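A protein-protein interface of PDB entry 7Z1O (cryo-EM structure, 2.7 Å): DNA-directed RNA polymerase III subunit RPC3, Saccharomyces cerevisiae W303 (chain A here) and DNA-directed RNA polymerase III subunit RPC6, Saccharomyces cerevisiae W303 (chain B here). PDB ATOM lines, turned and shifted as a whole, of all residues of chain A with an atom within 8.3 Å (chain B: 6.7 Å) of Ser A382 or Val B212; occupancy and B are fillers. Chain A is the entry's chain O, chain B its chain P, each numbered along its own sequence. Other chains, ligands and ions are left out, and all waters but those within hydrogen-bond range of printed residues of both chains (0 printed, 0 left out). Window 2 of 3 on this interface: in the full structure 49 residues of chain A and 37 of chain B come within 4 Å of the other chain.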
ATOM      1  N   SER A 379      22.270  29.258 -14.764  1.00  0.00           N
ATOM      2  CA  SER A 379      22.649  27.971 -15.334  1.00  0.00           C
ATOM      3  C   SER A 379      23.767  28.077 -16.364  1.00  0.00           C
ATOM      4  O   SER A 379      24.358  27.052 -16.716  1.00  0.00           O
ATOM      5  CB  SER A 379      21.428  27.304 -15.969  1.00  0.00           C
ATOM      6  OG  SER A 379      21.776  26.064 -16.561  1.00  0.00           O
ATOM      7  N   LEU A 380      24.072  29.276 -16.857  1.00  0.00           N
ATOM      8  CA  LEU A 380      25.060  29.452 -17.913  1.00  0.00           C
ATOM      9  C   LEU A 380      26.145  30.428 -17.482  1.00  0.00           C
ATOM     10  O   LEU A 380      25.874  31.406 -16.777  1.00  0.00           O
ATOM     11  CB  LEU A 380      24.423  29.960 -19.214  1.00  0.00           C
ATOM     12  CG  LEU A 380      23.777  28.977 -20.199  1.00  0.00           C
ATOM     13  CD1 LEU A 380      24.822  28.015 -20.737  1.00  0.00           C
ATOM     14  CD2 LEU A 380      22.593  28.230 -19.616  1.00  0.00           C
ATOM     15  N   LEU A 381      27.374  30.153 -17.913  1.00  0.00           N
ATOM     16  CA  LEU A 381      28.497  31.074 -17.778  1.00  0.00           C
ATOM     17  C   LEU A 381      28.918  31.512 -19.174  1.00  0.00           C
ATOM     18  O   LEU A 381      29.264  30.674 -20.014  1.00  0.00           O
ATOM     19  CB  LEU A 381      29.669  30.429 -17.037  1.00  0.00           C
ATOM     20  CG  LEU A 381      29.733  30.472 -15.503  1.00  0.00           C
ATOM     21  CD1 LEU A 381      30.105  31.872 -15.028  1.00  0.00           C
ATOM     22  CD2 LEU A 381      28.452  29.995 -14.827  1.00  0.00           C
ATOM     23  N   SER A 382      28.890  32.825 -19.417  1.00  0.00           N
ATOM     24  CA  SER A 382      29.144  33.334 -20.762  1.00  0.00           C
ATOM     25  C   SER A 382      30.626  33.316 -21.116  1.00  0.00           C
ATOM     26  O   SER A 382      30.974  33.235 -22.298  1.00  0.00           O
ATOM     27  CB  SER A 382      28.585  34.749 -20.899  1.00  0.00           C
ATOM     28  OG  SER A 382      27.180  34.761 -20.721  1.00  0.00           O
ATOM     29  N   ARG A 383      31.508  33.402 -20.123  1.00  0.00           N
ATOM     30  CA  ARG A 383      32.941  33.458 -20.364  1.00  0.00           C
ATOM     31  C   ARG A 383      33.670  32.526 -19.406  1.00  0.00           C
ATOM     32  O   ARG A 383      33.170  32.203 -18.325  1.00  0.00           O
ATOM     33  CB  ARG A 383      33.481  34.887 -20.214  1.00  0.00           C
ATOM     34  CG  ARG A 383      33.305  35.479 -18.825  1.00  0.00           C
ATOM     35  CD  ARG A 383      33.872  36.887 -18.752  1.00  0.00           C
ATOM     36  NE  ARG A 383      33.159  37.810 -19.628  1.00  0.00           N
ATOM     37  CZ  ARG A 383      32.047  38.450 -19.296  1.00  0.00           C
ATOM     38  NH1 ARG A 383      31.488  38.294 -18.107  1.00  0.00           N
ATOM     39  NH2 ARG A 383      31.480  39.268 -20.179  1.00  0.00           N
ATOM     40  N   LYS A 384      34.858  32.097 -19.820  1.00  0.00           N
ATOM     41  CA  LYS A 384      35.684  31.210 -19.008  1.00  0.00           C
ATOM     42  C   LYS A 384      36.252  31.942 -17.797  1.00  0.00           C
ATOM     43  O   LYS A 384      37.125  31.424 -17.101  1.00  0.00           O
ATOM     44  CB  LYS A 384      36.821  30.622 -19.846  1.00  0.00           C
ATOM     45  CG  LYS A 384      36.365  29.610 -20.881  1.00  0.00           C
ATOM     46  CD  LYS A 384      37.524  29.116 -21.730  1.00  0.00           C
ATOM     47  CE  LYS A 384      38.370  28.104 -20.977  1.00  0.00           C
ATOM     48  NZ  LYS A 384      37.618  26.849 -20.706  1.00  0.00           N
ATOM     49  N   SER A 451      16.084  34.734 -24.112  1.00  0.00           N
ATOM     50  CA  SER A 451      17.498  34.559 -24.432  1.00  0.00           C
ATOM     51  C   SER A 451      18.072  33.308 -23.778  1.00  0.00           C
ATOM     52  O   SER A 451      18.872  32.590 -24.389  1.00  0.00           O
ATOM     53  CB  SER A 451      18.288  35.796 -24.008  1.00  0.00           C
ATOM     54  OG  SER A 451      19.678  35.523 -23.970  1.00  0.00           O
ATOM     55  N   LEU A 452      17.680  33.033 -22.533  1.00  0.00           N
ATOM     56  CA  LEU A 452      18.183  31.852 -21.838  1.00  0.00           C
ATOM     57  C   LEU A 452      17.670  30.568 -22.481  1.00  0.00           C
ATOM     58  O   LEU A 452      18.420  29.593 -22.633  1.00  0.00           O
ATOM     59  CB  LEU A 452      17.794  31.922 -20.363  1.00  0.00           C
ATOM     60  CG  LEU A 452      18.548  32.990 -19.569  1.00  0.00           C
ATOM     61  CD1 LEU A 452      17.883  33.244 -18.228  1.00  0.00           C
ATOM     62  CD2 LEU A 452      20.004  32.589 -19.383  1.00  0.00           C
ATOM     63  N   SER A 455      19.631  30.076 -25.612  1.00  0.00           N
ATOM     64  CA  SER A 455      20.957  29.537 -25.320  1.00  0.00           C
ATOM     65  C   SER A 455      20.898  28.042 -25.025  1.00  0.00           C
ATOM     66  O   SER A 455      21.742  27.273 -25.506  1.00  0.00           O
ATOM     67  CB  SER A 455      21.584  30.290 -24.148  1.00  0.00           C
ATOM     68  OG  SER A 455      21.849  31.638 -24.493  1.00  0.00           O
ATOM     69  N   SER A 462      23.811  22.227 -30.909  1.00  0.00           N
ATOM     70  CA  SER A 462      25.235  22.137 -31.203  1.00  0.00           C
ATOM     71  C   SER A 462      25.889  20.899 -30.607  1.00  0.00           C
ATOM     72  O   SER A 462      27.106  20.734 -30.742  1.00  0.00           O
ATOM     73  CB  SER A 462      25.960  23.389 -30.702  1.00  0.00           C
ATOM     74  OG  SER A 462      27.359  23.174 -30.631  1.00  0.00           O
ATOM     75  N   PHE B 207      27.191  24.978 -16.748  1.00  0.00           N
ATOM     76  CA  PHE B 207      27.870  24.594 -17.977  1.00  0.00           C
ATOM     77  C   PHE B 207      28.197  25.849 -18.778  1.00  0.00           C
ATOM     78  O   PHE B 207      27.666  26.934 -18.522  1.00  0.00           O
ATOM     79  CB  PHE B 207      27.020  23.624 -18.809  1.00  0.00           C
ATOM     80  CG  PHE B 207      26.682  22.346 -18.096  1.00  0.00           C
ATOM     81  CD1 PHE B 207      25.560  22.260 -17.289  1.00  0.00           C
ATOM     82  CD2 PHE B 207      27.487  21.229 -18.236  1.00  0.00           C
ATOM     83  CE1 PHE B 207      25.252  21.088 -16.631  1.00  0.00           C
ATOM     84  CE2 PHE B 207      27.181  20.053 -17.581  1.00  0.00           C
ATOM     85  CZ  PHE B 207      26.063  19.982 -16.779  1.00  0.00           C
ATOM     86  N   TYR B 208      29.079  25.695 -19.759  1.00  0.00           N
ATOM     87  CA  TYR B 208      29.499  26.814 -20.588  1.00  0.00           C
ATOM     88  C   TYR B 208      28.428  27.185 -21.605  1.00  0.00           C
ATOM     89  O   TYR B 208      27.608  26.358 -22.013  1.00  0.00           O
ATOM     90  CB  TYR B 208      30.803  26.488 -21.314  1.00  0.00           C
ATOM     91  CG  TYR B 208      32.045  26.701 -20.482  1.00  0.00           C
ATOM     92  CD1 TYR B 208      32.007  27.465 -19.323  1.00  0.00           C
ATOM     93  CD2 TYR B 208      33.258  26.142 -20.856  1.00  0.00           C
ATOM     94  CE1 TYR B 208      33.141  27.666 -18.564  1.00  0.00           C
ATOM     95  CE2 TYR B 208      34.396  26.334 -20.102  1.00  0.00           C
ATOM     96  CZ  TYR B 208      34.332  27.096 -18.957  1.00  0.00           C
ATOM     97  OH  TYR B 208      35.465  27.291 -18.203  1.00  0.00           O
ATOM     98  N   ALA B 209      28.449  28.451 -22.010  1.00  0.00           N
ATOM     99  CA  ALA B 209      27.591  28.928 -23.077  1.00  0.00           C
ATOM    100  C   ALA B 209      28.034  28.319 -24.408  1.00  0.00           C
ATOM    101  O   ALA B 209      29.191  27.918 -24.556  1.00  0.00           O
ATOM    102  CB  ALA B 209      27.631  30.455 -23.133  1.00  0.00           C
ATOM    103  N   PRO B 210      27.123  28.207 -25.382  1.00  0.00           N
ATOM    104  CA  PRO B 210      27.496  27.578 -26.663  1.00  0.00           C
ATOM    105  C   PRO B 210      28.603  28.298 -27.418  1.00  0.00           C
ATOM    106  O   PRO B 210      29.353  27.647 -28.155  1.00  0.00           O
ATOM    107  CB  PRO B 210      26.180  27.588 -27.456  1.00  0.00           C
ATOM    108  CG  PRO B 210      25.316  28.591 -26.771  1.00  0.00           C
ATOM    109  CD  PRO B 210      25.685  28.519 -25.331  1.00  0.00           C
ATOM    110  N   ASN B 211      28.732  29.617 -27.261  1.00  0.00           N
ATOM    111  CA  ASN B 211      29.779  30.341 -27.972  1.00  0.00           C
ATOM    112  C   ASN B 211      31.158  30.132 -27.357  1.00  0.00           C
ATOM    113  O   ASN B 211      32.162  30.489 -27.981  1.00  0.00           O
ATOM    114  CB  ASN B 211      29.448  31.836 -28.024  1.00  0.00           C
ATOM    115  CG  ASN B 211      29.123  32.414 -26.658  1.00  0.00           C
ATOM    116  OD1 ASN B 211      29.254  31.742 -25.638  1.00  0.00           O
ATOM    117  ND2 ASN B 211      28.696  33.670 -26.637  1.00  0.00           N
ATOM    118  N   VAL B 212      31.228  29.566 -26.155  1.00  0.00           N
ATOM    119  CA  VAL B 212      32.501  29.331 -25.485  1.00  0.00           C
ATOM    120  C   VAL B 212      33.200  28.139 -26.123  1.00  0.00           C
ATOM    121  O   VAL B 212      32.581  27.102 -26.389  1.00  0.00           O
ATOM    122  CB  VAL B 212      32.281  29.107 -23.979  1.00  0.00           C
ATOM    123  CG1 VAL B 212      33.606  29.104 -23.244  1.00  0.00           C
ATOM    124  CG2 VAL B 212      31.360  30.171 -23.417  1.00  0.00           C
ATOM    125  N   LYS B 213      34.499  28.287 -26.376  1.00  0.00           N
ATOM    126  CA  LYS B 213      35.306  27.216 -26.962  1.00  0.00           C
ATOM    127  C   LYS B 213      35.775  26.270 -25.855  1.00  0.00           C
ATOM    128  O   LYS B 213      36.923  26.289 -25.409  1.00  0.00           O
ATOM    129  CB  LYS B 213      36.481  27.800 -27.737  1.00  0.00           C
ATOM    130  CG  LYS B 213      36.081  28.608 -28.959  1.00  0.00           C
ATOM    131  CD  LYS B 213      37.305  29.046 -29.748  1.00  0.00           C
ATOM    132  CE  LYS B 213      38.147  30.031 -28.953  1.00  0.00           C
ATOM    133  NZ  LYS B 213      39.303  30.540 -29.742  1.00  0.00           N
ATOM    134  N   ASN B 214      34.844  25.422 -25.414  1.00  0.00           N
ATOM    135  CA  ASN B 214      35.140  24.491 -24.331  1.00  0.00           C
ATOM    136  C   ASN B 214      35.991  23.314 -24.786  1.00  0.00           C
ATOM    137  O   ASN B 214      36.554  22.613 -23.940  1.00  0.00           O
ATOM    138  CB  ASN B 214      33.841  23.986 -23.700  1.00  0.00           C
ATOM    139  CG  ASN B 214      32.848  23.472 -24.727  1.00  0.00           C
ATOM    140  OD1 ASN B 214      33.156  23.370 -25.914  1.00  0.00           O
ATOM    141  ND2 ASN B 214      31.644  23.148 -24.271  1.00  0.00           N
ATOM    142  N   TYR B 215      36.100  23.080 -26.091  1.00  0.00           N
ATOM    143  CA  TYR B 215      36.890  21.962 -26.584  1.00  0.00           C
ATOM    144  C   TYR B 215      38.379  22.217 -26.378  1.00  0.00           C
ATOM    145  O   TYR B 215      38.862  23.348 -26.484  1.00  0.00           O
ATOM    146  CB  TYR B 215      36.597  21.709 -28.065  1.00  0.00           C
ATOM    147  CG  TYR B 215      36.884  22.881 -28.981  1.00  0.00           C
ATOM    148  CD1 TYR B 215      35.915  23.844 -29.232  1.00  0.00           C
ATOM    149  CD2 TYR B 215      38.117  23.015 -29.607  1.00  0.00           C
ATOM    150  CE1 TYR B 215      36.170  24.912 -30.069  1.00  0.00           C
ATOM    151  CE2 TYR B 215      38.381  24.080 -30.445  1.00  0.00           C
ATOM    152  CZ  TYR B 215      37.404  25.025 -30.673  1.00  0.00           C
ATOM    153  OH  TYR B 215      37.662  26.087 -31.509  1.00  0.00           O
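N of Leu A381 is in hydrogen-bond range of O of Phe B207. The backbone carbonyl oxygen (O) of Leu A381 is in hydrogen-bond range of the backbone NH (N) of Ala B209, 3.1 Å away. The side-chain hydroxyl of Tyr B208 lies close to the side-chain amino group of Lys A384, 3.3 Å away.
Among the printed residues, merely in contact across the chains: Ser A382 with Val B212, Leu A380 with Tyr B208, Ser A379 with Phe B207, Lys A384 with Val B212, Leu A380 with Phe B207, Leu A380 with Ala B209 and Leu A381 with Tyr B208.
Of chain B, only Val B212 (3.3 Å) comes within 4 Å of Ser A382. Ala B209 touches just these residues of chain A: Leu A380 and Leu A381. Of the printed residues of chain A, Phe B207 touches Ser A379, Leu A380 and Leu A381. Of the printed residues of chain B, Leu A381 touches Phe B207, Tyr B208 and Ala B209. Of the printed residues of chain A, Tyr B208 touches Leu A380 (3.5 Å), Leu A381 (3.9 Å) and Lys A384 (3.3 Å). Printed residues of chain B within 4 Å of Leu A380: Phe B207, Tyr B208 and Ala B209. Printed residues of chain B within 4 Å of Lys A384: Tyr B208 and Val B212. Ser A462 touches none of the printed residues of chain B. Pro B210 touches none of the printed residues of chain A. The nearest printed residue of chain B that does not touch Ser A382 is Ala B209 (4.02 Å). The nearest printed residue of chain B that does not touch Leu A381 is Val B212 (4.03 Å).
Of the 9 printed residues of chain B, 4 touch a printed residue of chain A. Printed residues of chain B that touch a printed residue of chain A: Phe B207, Tyr B208, Ala B209 and Val B212. Along chain B the printed residues that touch a printed residue of chain A span positions 207 to 212. Of the 10 printed residues of chain A, 5 touch a printed residue of chain B. Along chain A the printed residues that touch a printed residue of chain B span positions 379 to 384.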
